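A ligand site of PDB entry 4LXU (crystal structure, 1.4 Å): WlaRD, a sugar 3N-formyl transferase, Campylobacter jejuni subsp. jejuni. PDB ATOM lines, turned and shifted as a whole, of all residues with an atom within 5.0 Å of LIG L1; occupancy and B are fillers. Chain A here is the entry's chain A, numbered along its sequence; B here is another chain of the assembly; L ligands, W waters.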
ATOM      1  N   SER A  77      -4.568 -28.399 -35.161  1.00  0.00           N
ATOM      2  CA  SER A  77      -3.824 -29.287 -34.270  1.00  0.00           C
ATOM      3  C   SER A  77      -4.657 -30.524 -33.938  1.00  0.00           C
ATOM      4  O   SER A  77      -5.808 -30.448 -33.515  1.00  0.00           O
ATOM      5  CB  SER A  77      -3.571 -28.517 -32.982  1.00  0.00           C
ATOM      6  OG  SER A  77      -3.250 -29.425 -31.896  1.00  0.00           O
ATOM      7  N   PHE A  80      -1.103 -32.113 -31.522  1.00  0.00           N
ATOM      8  CA  PHE A  80       0.145 -31.379 -31.659  1.00  0.00           C
ATOM      9  C   PHE A  80       0.815 -31.097 -30.318  1.00  0.00           C
ATOM     10  O   PHE A  80       0.143 -30.818 -29.320  1.00  0.00           O
ATOM     11  CB  PHE A  80      -0.131 -30.052 -32.434  1.00  0.00           C
ATOM     12  CG  PHE A  80       1.051 -29.266 -32.872  1.00  0.00           C
ATOM     13  CD1 PHE A  80       1.082 -27.867 -32.688  1.00  0.00           C
ATOM     14  CD2 PHE A  80       2.107 -29.890 -33.517  1.00  0.00           C
ATOM     15  CE1 PHE A  80       2.165 -27.121 -33.182  1.00  0.00           C
ATOM     16  CE2 PHE A  80       3.203 -29.169 -33.996  1.00  0.00           C
ATOM     17  CZ  PHE A  80       3.210 -27.770 -33.864  1.00  0.00           C
ATOM     18  N   ASP A  81       2.136 -31.140 -30.357  1.00  0.00           N
ATOM     19  CA  ASP A  81       2.961 -31.085 -29.142  1.00  0.00           C
ATOM     20  C   ASP A  81       3.442 -29.710 -28.718  1.00  0.00           C
ATOM     21  O   ASP A  81       4.061 -29.556 -27.663  1.00  0.00           O
ATOM     22  CB  ASP A  81       4.150 -32.062 -29.173  1.00  0.00           C
ATOM     23  CG  ASP A  81       5.104 -31.795 -30.303  1.00  0.00           C
ATOM     24  OD1 ASP A  81       6.173 -32.462 -30.336  1.00  0.00           O
ATOM     25  OD2 ASP A  81       4.891 -30.894 -31.163  1.00  0.00           O
ATOM     26  N   GLN A  82       3.231 -28.710 -29.566  1.00  0.00           N
ATOM     27  CA  GLN A  82       3.719 -27.349 -29.258  1.00  0.00           C
ATOM     28  C   GLN A  82       2.612 -26.381 -28.918  1.00  0.00           C
ATOM     29  O   GLN A  82       1.622 -26.317 -29.644  1.00  0.00           O
ATOM     30  CB  GLN A  82       4.526 -26.750 -30.409  1.00  0.00           C
ATOM     31  CG  GLN A  82       5.729 -27.555 -30.886  1.00  0.00           C
ATOM     32  CD  GLN A  82       6.570 -26.817 -31.931  1.00  0.00           C
ATOM     33  OE1 GLN A  82       7.107 -25.759 -31.575  1.00  0.00           O
ATOM     34  NE2 GLN A  82       6.700 -27.341 -33.153  1.00  0.00           N
ATOM     35  N   ILE A  83       2.754 -25.625 -27.837  1.00  0.00           N
ATOM     36  CA  ILE A  83       1.881 -24.515 -27.472  1.00  0.00           C
ATOM     37  C   ILE A  83       2.169 -23.338 -28.406  1.00  0.00           C
ATOM     38  O   ILE A  83       3.301 -22.912 -28.470  1.00  0.00           O
ATOM     39  CB  ILE A  83       2.177 -24.119 -26.016  1.00  0.00           C
ATOM     40  CG1 ILE A  83       1.593 -25.211 -25.102  1.00  0.00           C
ATOM     41  CG2 ILE A  83       1.531 -22.772 -25.693  1.00  0.00           C
ATOM     42  CD1 ILE A  83       0.092 -25.175 -24.975  1.00  0.00           C
ATOM     43  N   ILE A  84       1.193 -22.916 -29.163  1.00  0.00           N
ATOM     44  CA  ILE A  84       1.394 -21.765 -30.087  1.00  0.00           C
ATOM     45  C   ILE A  84       0.993 -20.475 -29.387  1.00  0.00           C
ATOM     46  O   ILE A  84       0.226 -20.444 -28.406  1.00  0.00           O
ATOM     47  CB  ILE A  84       0.633 -21.973 -31.419  1.00  0.00           C
ATOM     48  CG1 ILE A  84      -0.873 -21.994 -31.246  1.00  0.00           C
ATOM     49  CG2 ILE A  84       1.053 -23.290 -32.159  1.00  0.00           C
ATOM     50  CD1 ILE A  84      -1.671 -21.781 -32.539  1.00  0.00           C
ATOM     51  N   ASN A  96      -8.182 -26.845 -32.643  1.00  0.00           N
ATOM     52  CA  ASN A  96      -7.652 -28.057 -31.973  1.00  0.00           C
ATOM     53  C   ASN A  96      -8.832 -28.950 -31.655  1.00  0.00           C
ATOM     54  O   ASN A  96      -9.955 -28.498 -31.393  1.00  0.00           O
ATOM     55  CB  ASN A  96      -6.934 -27.647 -30.675  1.00  0.00           C
ATOM     56  CG  ASN A  96      -6.427 -28.843 -29.883  1.00  0.00           C
ATOM     57  OD1 ASN A  96      -6.954 -29.097 -28.740  1.00  0.00           O
ATOM     58  ND2 ASN A  96      -5.478 -29.552 -30.407  1.00  0.00           N
ATOM     59  N   HIS A  98      -9.438 -31.434 -28.572  1.00  0.00           N
ATOM     60  CA  HIS A  98      -8.977 -31.805 -27.235  1.00  0.00           C
ATOM     61  C   HIS A  98      -9.654 -33.071 -26.778  1.00  0.00           C
ATOM     62  O   HIS A  98     -10.861 -33.227 -26.855  1.00  0.00           O
ATOM     63  CB  HIS A  98      -9.212 -30.661 -26.241  1.00  0.00           C
ATOM     64  CG  HIS A  98      -8.687 -31.016 -24.870  1.00  0.00           C
ATOM     65  ND1 HIS A  98      -7.333 -31.092 -24.602  1.00  0.00           N
ATOM     66  CD2 HIS A  98      -9.333 -31.324 -23.726  1.00  0.00           C
ATOM     67  CE1 HIS A  98      -7.167 -31.442 -23.324  1.00  0.00           C
ATOM     68  NE2 HIS A  98      -8.363 -31.567 -22.778  1.00  0.00           N
ATOM     69  N   GLY A 107      -5.237 -29.727 -20.268  1.00  0.00           N
ATOM     70  CA  GLY A 107      -3.861 -30.103 -19.995  1.00  0.00           C
ATOM     71  C   GLY A 107      -3.528 -31.444 -20.634  1.00  0.00           C
ATOM     72  O   GLY A 107      -3.835 -31.655 -21.814  1.00  0.00           O
ATOM     73  N   VAL A 108      -2.829 -32.304 -19.905  1.00  0.00           N
ATOM     74  CA  VAL A 108      -2.191 -33.493 -20.481  1.00  0.00           C
ATOM     75  C   VAL A 108      -2.683 -34.751 -19.761  1.00  0.00           C
ATOM     76  O   VAL A 108      -3.488 -34.690 -18.816  1.00  0.00           O
ATOM     77  CB  VAL A 108      -0.672 -33.373 -20.413  1.00  0.00           C
ATOM     78  CG1 VAL A 108      -0.207 -32.073 -21.194  1.00  0.00           C
ATOM     79  CG2 VAL A 108      -0.207 -33.409 -18.988  1.00  0.00           C
ATOM     80  N   HIS A 127     -12.344 -27.027 -30.576  1.00  0.00           N
ATOM     81  CA  HIS A 127     -12.325 -25.643 -30.082  1.00  0.00           C
ATOM     82  C   HIS A 127     -11.353 -24.758 -30.851  1.00  0.00           C
ATOM     83  O   HIS A 127     -10.440 -25.234 -31.512  1.00  0.00           O
ATOM     84  CB  HIS A 127     -12.063 -25.637 -28.563  1.00  0.00           C
ATOM     85  CG  HIS A 127     -10.688 -26.117 -28.175  1.00  0.00           C
ATOM     86  ND1 HIS A 127      -9.601 -25.290 -28.037  1.00  0.00           N
ATOM     87  CD2 HIS A 127     -10.220 -27.379 -27.964  1.00  0.00           C
ATOM     88  CE1 HIS A 127      -8.515 -25.981 -27.726  1.00  0.00           C
ATOM     89  NE2 HIS A 127      -8.886 -27.262 -27.663  1.00  0.00           N
ATOM     90  N   ILE A 129      -8.167 -22.397 -30.878  1.00  0.00           N
ATOM     91  CA  ILE A 129      -6.965 -22.205 -30.082  1.00  0.00           C
ATOM     92  C   ILE A 129      -6.849 -20.740 -29.700  1.00  0.00           C
ATOM     93  O   ILE A 129      -6.863 -19.865 -30.583  1.00  0.00           O
ATOM     94  CB  ILE A 129      -5.695 -22.645 -30.817  1.00  0.00           C
ATOM     95  CG1 ILE A 129      -5.751 -24.169 -31.122  1.00  0.00           C
ATOM     96  CG2 ILE A 129      -4.408 -22.281 -30.086  1.00  0.00           C
ATOM     97  CD1 ILE A 129      -4.578 -24.698 -31.935  1.00  0.00           C
ATOM     98  N   ASP A 130      -6.738 -20.447 -28.408  1.00  0.00           N
ATOM     99  CA  ASP A 130      -6.293 -19.161 -27.886  1.00  0.00           C
ATOM    100  C   ASP A 130      -4.986 -19.333 -27.158  1.00  0.00           C
ATOM    101  O   ASP A 130      -4.380 -20.409 -27.274  1.00  0.00           O
ATOM    102  CB  ASP A 130      -7.393 -18.478 -27.077  1.00  0.00           C
ATOM    103  CG  ASP A 130      -7.741 -19.184 -25.783  1.00  0.00           C
ATOM    104  OD1 ASP A 130      -8.805 -18.847 -25.226  1.00  0.00           O
ATOM    105  OD2 ASP A 130      -6.947 -20.038 -25.368  1.00  0.00           O
ATOM    106  N   ASN A 131      -4.429 -18.310 -26.499  1.00  0.00           N
ATOM    107  CA  ASN A 131      -3.096 -18.469 -25.950  1.00  0.00           C
ATOM    108  C   ASN A 131      -2.985 -19.356 -24.695  1.00  0.00           C
ATOM    109  O   ASN A 131      -1.849 -19.685 -24.352  1.00  0.00           O
ATOM    110  CB  ASN A 131      -2.540 -17.095 -25.596  1.00  0.00           C
ATOM    111  CG  ASN A 131      -1.946 -16.434 -26.834  1.00  0.00           C
ATOM    112  OD1 ASN A 131      -1.533 -17.061 -27.816  1.00  0.00           O
ATOM    113  ND2 ASN A 131      -1.985 -15.116 -26.780  1.00  0.00           N
ATOM    114  N   GLY A 132      -4.109 -19.710 -24.106  1.00  0.00           N
ATOM    115  CA  GLY A 132      -4.096 -20.681 -22.987  1.00  0.00           C
ATOM    116  C   GLY A 132      -4.130 -22.107 -23.489  1.00  0.00           C
ATOM    117  O   GLY A 132      -4.416 -22.418 -24.652  1.00  0.00           O
ATOM    118  N   ILE A 133      -3.968 -22.994 -22.513  1.00  0.00           N
ATOM    119  CA  ILE A 133      -3.995 -24.455 -22.782  1.00  0.00           C
ATOM    120  C   ILE A 133      -5.441 -24.996 -22.697  1.00  0.00           C
ATOM    121  O   ILE A 133      -6.043 -25.078 -21.619  1.00  0.00           O
ATOM    122  CB  ILE A 133      -3.048 -25.156 -21.782  1.00  0.00           C
ATOM    123  CG1 ILE A 133      -1.593 -24.704 -21.926  1.00  0.00           C
ATOM    124  CG2 ILE A 133      -3.140 -26.698 -22.077  1.00  0.00           C
ATOM    125  CD1 ILE A 133      -0.613 -25.208 -20.903  1.00  0.00           C
ATOM    126  N   ASP A 134      -6.004 -25.320 -23.853  1.00  0.00           N
ATOM    127  CA  ASP A 134      -7.331 -25.893 -24.015  1.00  0.00           C
ATOM    128  C   ASP A 134      -8.446 -25.009 -23.481  1.00  0.00           C
ATOM    129  O   ASP A 134      -9.490 -25.482 -23.053  1.00  0.00           O
ATOM    130  CB  ASP A 134      -7.424 -27.284 -23.315  1.00  0.00           C
ATOM    131  CG  ASP A 134      -6.300 -28.209 -23.715  1.00  0.00           C
ATOM    132  OD1 ASP A 134      -5.937 -28.270 -24.921  1.00  0.00           O
ATOM    133  OD2 ASP A 134      -5.741 -28.903 -22.805  1.00  0.00           O
ATOM    134  N   THR A 135      -8.218 -23.685 -23.603  1.00  0.00           N
ATOM    135  CA  THR A 135      -9.087 -22.678 -23.021  1.00  0.00           C
ATOM    136  C   THR A 135      -9.999 -21.987 -24.041  1.00  0.00           C
ATOM    137  O   THR A 135     -10.960 -21.285 -23.619  1.00  0.00           O
ATOM    138  CB  THR A 135      -8.222 -21.591 -22.303  1.00  0.00           C
ATOM    139  OG1 THR A 135      -7.084 -21.322 -23.133  1.00  0.00           O
ATOM    140  CG2 THR A 135      -7.659 -22.126 -20.954  1.00  0.00           C
ATOM    141  N   TYR A 191      -7.637 -28.870 -14.753  1.00  0.00           N
ATOM    142  CA  TYR A 191      -6.418 -28.865 -15.532  1.00  0.00           C
ATOM    143  C   TYR A 191      -5.409 -29.731 -14.815  1.00  0.00           C
ATOM    144  O   TYR A 191      -5.265 -29.651 -13.599  1.00  0.00           O
ATOM    145  CB  TYR A 191      -5.845 -27.439 -15.649  1.00  0.00           C
ATOM    146  CG  TYR A 191      -4.438 -27.332 -16.183  1.00  0.00           C
ATOM    147  CD1 TYR A 191      -4.194 -27.280 -17.553  1.00  0.00           C
ATOM    148  CD2 TYR A 191      -3.351 -27.215 -15.330  1.00  0.00           C
ATOM    149  CE1 TYR A 191      -2.931 -27.142 -18.051  1.00  0.00           C
ATOM    150  CE2 TYR A 191      -2.095 -27.091 -15.791  1.00  0.00           C
ATOM    151  CZ  TYR A 191      -1.856 -27.011 -17.185  1.00  0.00           C
ATOM    152  OH  TYR A 191      -0.570 -26.887 -17.648  1.00  0.00           O
ATOM    153  N   PHE A 192      -4.662 -30.530 -15.592  1.00  0.00           N
ATOM    154  CA  PHE A 192      -3.578 -31.312 -15.015  1.00  0.00           C
ATOM    155  C   PHE A 192      -2.364 -31.140 -15.905  1.00  0.00           C
ATOM    156  O   PHE A 192      -2.471 -31.297 -17.121  1.00  0.00           O
ATOM    157  CB  PHE A 192      -3.968 -32.807 -14.930  1.00  0.00           C
ATOM    158  CG  PHE A 192      -5.098 -33.034 -13.969  1.00  0.00           C
ATOM    159  CD1 PHE A 192      -4.848 -33.327 -12.636  1.00  0.00           C
ATOM    160  CD2 PHE A 192      -6.395 -32.828 -14.381  1.00  0.00           C
ATOM    161  CE1 PHE A 192      -5.881 -33.421 -11.742  1.00  0.00           C
ATOM    162  CE2 PHE A 192      -7.446 -32.934 -13.498  1.00  0.00           C
ATOM    163  CZ  PHE A 192      -7.177 -33.247 -12.173  1.00  0.00           C
ATOM    164  N   SER A 193      -1.218 -30.912 -15.289  1.00  0.00           N
ATOM    165  CA  SER A 193       0.061 -30.837 -15.981  1.00  0.00           C
ATOM    166  C   SER A 193       0.857 -32.112 -15.796  1.00  0.00           C
ATOM    167  O   SER A 193       0.480 -32.925 -14.949  1.00  0.00           O
ATOM    168  CB  SER A 193       0.909 -29.616 -15.622  1.00  0.00           C
ATOM    169  OG  SER A 193       1.267 -29.674 -14.262  1.00  0.00           O
ATOM    170  N   ARG A 194       1.977 -32.261 -16.488  1.00  0.00           N
ATOM    171  CA  ARG A 194       2.748 -33.500 -16.395  1.00  0.00           C
ATOM    172  C   ARG A 194       3.177 -33.722 -14.952  1.00  0.00           C
ATOM    173  O   ARG A 194       3.122 -34.854 -14.471  1.00  0.00           O
ATOM    174  CB  ARG A 194       3.912 -33.522 -17.392  1.00  0.00           C
ATOM    175  CG  ARG A 194       3.572 -33.325 -18.889  1.00  0.00           C
ATOM    176  CD  ARG A 194       3.226 -34.614 -19.675  1.00  0.00           C
ATOM    177  NE  ARG A 194       3.006 -34.452 -21.112  1.00  0.00           N
ATOM    178  CZ  ARG A 194       2.264 -35.256 -21.854  1.00  0.00           C
ATOM    179  NH1 ARG A 194       2.101 -35.039 -23.151  1.00  0.00           N
ATOM    180  NH2 ARG A 194       1.717 -36.353 -21.312  1.00  0.00           N
ATOM    181  N   LYS A 195       3.546 -32.674 -14.221  1.00  0.00           N
ATOM    182  CA  LYS A 195       4.019 -32.811 -12.849  1.00  0.00           C
ATOM    183  C   LYS A 195       2.933 -33.322 -11.918  1.00  0.00           C
ATOM    184  O   LYS A 195       3.246 -33.760 -10.819  1.00  0.00           O
ATOM    185  CB  LYS A 195       4.552 -31.477 -12.290  1.00  0.00           C
ATOM    186  CG  LYS A 195       3.495 -30.583 -11.631  1.00  0.00           C
ATOM    187  CD  LYS A 195       4.018 -29.235 -11.127  1.00  0.00           C
ATOM    188  CE  LYS A 195       2.851 -28.385 -10.671  1.00  0.00           C
ATOM    189  NZ  LYS A 195       1.926 -28.149 -11.807  1.00  0.00           N
ATOM    190  N   LYS B 206      -0.651 -23.913 -10.597  1.00  0.00           N
ATOM    191  CA  LYS B 206      -0.704 -24.353 -12.011  1.00  0.00           C
ATOM    192  C   LYS B 206      -1.984 -25.150 -12.239  1.00  0.00           C
ATOM    193  O   LYS B 206      -1.925 -26.347 -12.523  1.00  0.00           O
ATOM    194  CB  LYS B 206       0.563 -25.109 -12.412  1.00  0.00           C
ATOM    195  CG  LYS B 206       1.789 -24.220 -12.274  1.00  0.00           C
ATOM    196  CD  LYS B 206       2.952 -24.419 -13.249  1.00  0.00           C
ATOM    197  CE  LYS B 206       3.809 -23.140 -13.298  1.00  0.00           C
ATOM    198  NZ  LYS B 206       3.353 -22.212 -14.375  1.00  0.00           N
HETATM  199  N1  LIG L   1      -1.517 -23.963 -28.382  1.00  0.00           N
HETATM  200  C1  LIG L   1      -2.291 -23.242 -27.554  1.00  0.00           C
HETATM  201  N2  LIG L   1      -1.955 -21.931 -27.323  1.00  0.00           N
HETATM  202  N3  LIG L   1      -3.410 -23.668 -26.953  1.00  0.00           N
HETATM  203  C2  LIG L   1      -3.731 -24.964 -27.096  1.00  0.00           C
HETATM  204  O1  LIG L   1      -4.903 -25.258 -26.513  1.00  0.00           O
HETATM  205  C3  LIG L   1      -2.985 -25.797 -27.915  1.00  0.00           C
HETATM  206  N4  LIG L   1      -3.181 -27.213 -27.980  1.00  0.00           N
HETATM  207  C4  LIG L   1      -1.999 -27.969 -28.451  1.00  0.00           C
HETATM  208  C5  LIG L   1      -1.474 -27.317 -29.728  1.00  0.00           C
HETATM  209  N5  LIG L   1      -1.079 -25.936 -29.410  1.00  0.00           N
HETATM  210  C6  LIG L   1      -1.857 -25.259 -28.541  1.00  0.00           C
HETATM  211  C7  LIG L   1      -0.790 -28.150 -27.520  1.00  0.00           C
HETATM  212  N6  LIG L   1      -1.155 -28.881 -26.299  1.00  0.00           N
HETATM  213  C8  LIG L   1       1.739 -28.960 -23.265  1.00  0.00           C
HETATM  214  C9  LIG L   1       2.117 -28.877 -24.599  1.00  0.00           C
HETATM  215  C10 LIG L   1       1.169 -28.851 -25.636  1.00  0.00           C
HETATM  216  C11 LIG L   1      -0.188 -28.895 -25.342  1.00  0.00           C
HETATM  217  C12 LIG L   1      -0.578 -29.023 -24.002  1.00  0.00           C
HETATM  218  C13 LIG L   1       0.371 -29.009 -22.983  1.00  0.00           C
HETATM  219  C14 LIG L   1       2.758 -28.918 -22.182  1.00  0.00           C
HETATM  220  O2  LIG L   1       3.937 -28.983 -22.478  1.00  0.00           O
HETATM  221  N7  LIG L   1       2.346 -28.760 -20.932  1.00  0.00           N
HETATM  222  C15 LIG L   1       3.304 -28.613 -19.823  1.00  0.00           C
HETATM  223  C16 LIG L   1       2.983 -27.284 -19.106  1.00  0.00           C
HETATM  224  C17 LIG L   1       3.343 -26.070 -19.991  1.00  0.00           C
HETATM  225  C18 LIG L   1       3.182 -24.754 -19.269  1.00  0.00           C
HETATM  226  O3  LIG L   1       2.877 -24.704 -18.053  1.00  0.00           O
HETATM  227  O4  LIG L   1       3.386 -23.720 -19.970  1.00  0.00           O
HETATM  228  C19 LIG L   1       3.185 -29.696 -18.782  1.00  0.00           C
HETATM  229  O5  LIG L   1       2.083 -30.246 -18.630  1.00  0.00           O
HETATM  230  O6  LIG L   1       4.231 -29.955 -18.145  1.00  0.00           O
HETATM  231  C20 LIG L   1      -4.145 -27.886 -27.463  1.00  0.00           C
HETATM  232  O7  LIG L   1      -4.068 -29.145 -27.454  1.00  0.00           O
HETATM  233  O1  LG2 L   2      -2.837 -37.296 -23.574  1.00  0.00           O
HETATM  234  P1  LG2 L   2      -1.562 -36.619 -23.734  1.00  0.00           P
HETATM  235  O2  LG2 L   2      -0.628 -36.354 -22.639  1.00  0.00           O
HETATM  236  O3  LG2 L   2      -1.973 -35.184 -24.391  1.00  0.00           O
HETATM  237  C1  LG2 L   2      -1.022 -34.119 -24.432  1.00  0.00           C
HETATM  238  O4  LG2 L   2       0.065 -34.312 -25.307  1.00  0.00           O
HETATM  239  C2  LG2 L   2      -0.328 -34.447 -26.681  1.00  0.00           C
HETATM  240  C3  LG2 L   2       0.946 -34.767 -27.424  1.00  0.00           C
HETATM  241  C4  LG2 L   2      -1.796 -32.850 -24.835  1.00  0.00           C
HETATM  242  O5  LG2 L   2      -3.011 -32.862 -24.073  1.00  0.00           O
HETATM  243  C5  LG2 L   2      -2.188 -32.861 -26.298  1.00  0.00           C
HETATM  244  N1  LG2 L   2      -2.711 -31.503 -26.659  1.00  0.00           N
HETATM  245  C6  LG2 L   2      -0.930 -33.101 -27.138  1.00  0.00           C
HETATM  246  O6  LG2 L   2       0.020 -32.041 -26.984  1.00  0.00           O
HETATM  247  O7  LG2 L   2      -0.835 -37.275 -24.989  1.00  0.00           O
HETATM  248  P2  LG2 L   2       0.351 -38.335 -25.187  1.00  0.00           P
HETATM  249  O8  LG2 L   2       0.285 -38.647 -26.661  1.00  0.00           O
HETATM  250  O9  LG2 L   2       1.679 -37.976 -24.657  1.00  0.00           O
HETATM  251  O10 LG2 L   2      -0.161 -39.606 -24.342  1.00  0.00           O
HETATM  252  C7  LG2 L   2      -1.424 -40.180 -24.711  1.00  0.00           C
HETATM  253  C8  LG2 L   2      -1.925 -41.014 -23.550  1.00  0.00           C
HETATM  254  O11 LG2 L   2      -0.972 -42.080 -23.313  1.00  0.00           O
HETATM  255  C9  LG2 L   2      -1.979 -40.203 -22.277  1.00  0.00           C
HETATM  256  O12 LG2 L   2      -3.222 -39.534 -22.067  1.00  0.00           O
HETATM  257  C10 LG2 L   2      -1.902 -41.347 -21.233  1.00  0.00           C
HETATM  258  C11 LG2 L   2      -0.910 -42.278 -21.905  1.00  0.00           C
HETATM  259  N2  LG2 L   2       0.476 -42.183 -21.445  1.00  0.00           N
HETATM  260  C12 LG2 L   2       0.940 -42.994 -20.452  1.00  0.00           C
HETATM  261  O13 LG2 L   2       0.120 -43.729 -19.900  1.00  0.00           O
HETATM  262  N3  LG2 L   2       2.226 -42.913 -20.058  1.00  0.00           N
HETATM  263  C13 LG2 L   2       1.315 -41.338 -22.063  1.00  0.00           C
HETATM  264  C14 LG2 L   2       2.655 -41.246 -21.715  1.00  0.00           C
HETATM  265  C15 LG2 L   2       3.595 -40.276 -22.417  1.00  0.00           C
HETATM  266  C16 LG2 L   2       3.086 -42.104 -20.688  1.00  0.00           C
HETATM  267  O14 LG2 L   2       4.366 -42.114 -20.290  1.00  0.00           O
HETATM  268  O   HOH W   1      -6.758 -22.815 -26.378  1.00  0.00           O
HETATM  269  O   HOH W   2       5.191 -23.927 -22.153  1.00  0.00           O
HETATM  270  O   HOH W   3      -3.831 -30.003 -24.422  1.00  0.00           O
HETATM  271  O   HOH W   4       1.421 -26.147 -16.039  1.00  0.00           O
HETATM  272  O   HOH W   5      -0.195 -28.963 -19.598  1.00  0.00           O
HETATM  273  O   HOH W   6       4.385 -30.127 -15.467  1.00  0.00           O
HETATM  274  O   HOH W   7      -4.309 -31.888 -29.165  1.00  0.00           O
HETATM  275  O   HOH W   8      -5.850 -30.943 -26.753  1.00  0.00           O
HETATM  276  O   HOH W   9       6.800 -30.327 -19.190  1.00  0.00           O
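An oxygen (O5) of LIG L1 lies within hydrogen-bond range of the backbone NH (N) of Arg 194 (2.9 Å).
The backbone carbonyl oxygen of Asp 130 is in hydrogen-bond range of a nitrogen (N2) of LIG L1.
The backbone carbonyl oxygen (O) of Gln 82 sits at hydrogen-bond distance from a nitrogen (N5) of LIG L1, 2.7 Å away.
N of Ile 84 lies within hydrogen-bond range of N1 of LIG L1.
An oxygen (O6) of LG2 L2 sits at hydrogen-bond distance from the backbone carbonyl oxygen (O) of Phe 80 (2.6 Å).
The backbone carbonyl oxygen (O) of Gly 132 sits close to a nitrogen (N3) of LIG L1 (2.8 Å).
N of Asp 134 lies within hydrogen-bond range of O1 of LIG L1, at 2.9 Å.
NH2 of Arg 194 lies within salt-bridge range of O2 of LG2 L2, 2.7 Å away.
N2 of LIG L1 is in hydrogen-bond range of O of Ile 84 (2.9 Å).
OD1 of Asn 96 lies close to O7 of LIG L1 (3.2 Å).
The backbone carbonyl oxygen (O) of Gly 107 is in hydrogen-bond range of an oxygen (O5) of LG2 L2, 2.7 Å away.
An oxygen (O7) of LIG L1 lies within hydrogen-bond range of a nitrogen (N1) of LG2 L2 (2.8 Å).
ND2 of Asn 96 lies within hydrogen-bond range of OG of Ser 77 (2.7 Å).
N of Gly 107 lies within hydrogen-bond range of OD2 of Asp 134 (2.7 Å).
O of Phe 192 sits at hydrogen-bond distance from N of Val 108, 3.0 Å away.
The side-chain carboxylate (OD1) of Asp 134 sits at hydrogen-bond distance from a ring nitrogen (ND1) of His 98 (3.2 Å).
The backbone NH (N) of Phe 80 sits close to the side-chain hydroxyl (OG) of Ser 77 (3.5 Å).
N of His 98 sits at hydrogen-bond distance from OD1 of Asn 96, 3.4 Å away.
The side-chain carboxylate (OD2) of Asp 130 lies within hydrogen-bond range of the side-chain hydroxyl (OG1) of Thr 135, at 2.6 Å.
OD1 of Asn 96 sits at hydrogen-bond distance from NE2 of His 127.
Ser 77 touches LIG L1 (OG to C5, 3.5 Å).
O of Phe 80 touches C7 of LIG L1 (3.4 Å).
Asp 81 touches LIG L1.
CA of Ile 83 touches N1 of LIG L1, 3.6 Å away.
CG1 of Val 108 touches C13 of LIG L1, at 3.6 Å.
His 127 touches LIG L1.
Ile 129 touches LIG L1.
Asn 131 touches LIG L1 (O to N2, 3.7 Å).
C of Ile 133 touches O1 of LIG L1, at 3.9 Å.
Tyr 191 touches LIG L1.
Ser 193 touches LIG L1.
Hydrophobic or aromatic side chains within 4 Å of LIG L1: Phe 80, Ile 83, Ile 84, Val 108, His 127, Ile 129 and Ile 133.
Within 4 Å of LIG L1: Ser 77, Phe 80, Asp 81, Gln 82, Ile 83, Ile 84, Asn 96, Val 108, His 127, Ile 129, Asp 130, Asn 131, Gly 132, Ile 133, Asp 134, Tyr 191, Ser 193 and Arg 194.
The nearest printed residue that does not touch LIG L1 is Lys 206 of chain B (4.5 Å).
Water W6 lies within hydrogen-bond range of an oxygen (O6) of LIG L1 (2.7 Å), the backbone NH (N) of Lys 195 (3.0 Å), the side-chain hydroxyl (OG) of Ser 193 (3.4 Å) and the backbone NH (N) of Arg 194 (3.4 Å).
Water W5 lies within hydrogen-bond range of O5 of LIG L1 and OH of Tyr 191.
Water W4 lies within hydrogen-bond range of OH of Tyr 191 (2.7 Å) and O3 of LIG L1 (2.9 Å).
Water W7 lies within hydrogen-bond range of the side-chain amide nitrogen of Asn 96, a nitrogen (N1) of LG2 L2 and an oxygen (O7) of LIG L1.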
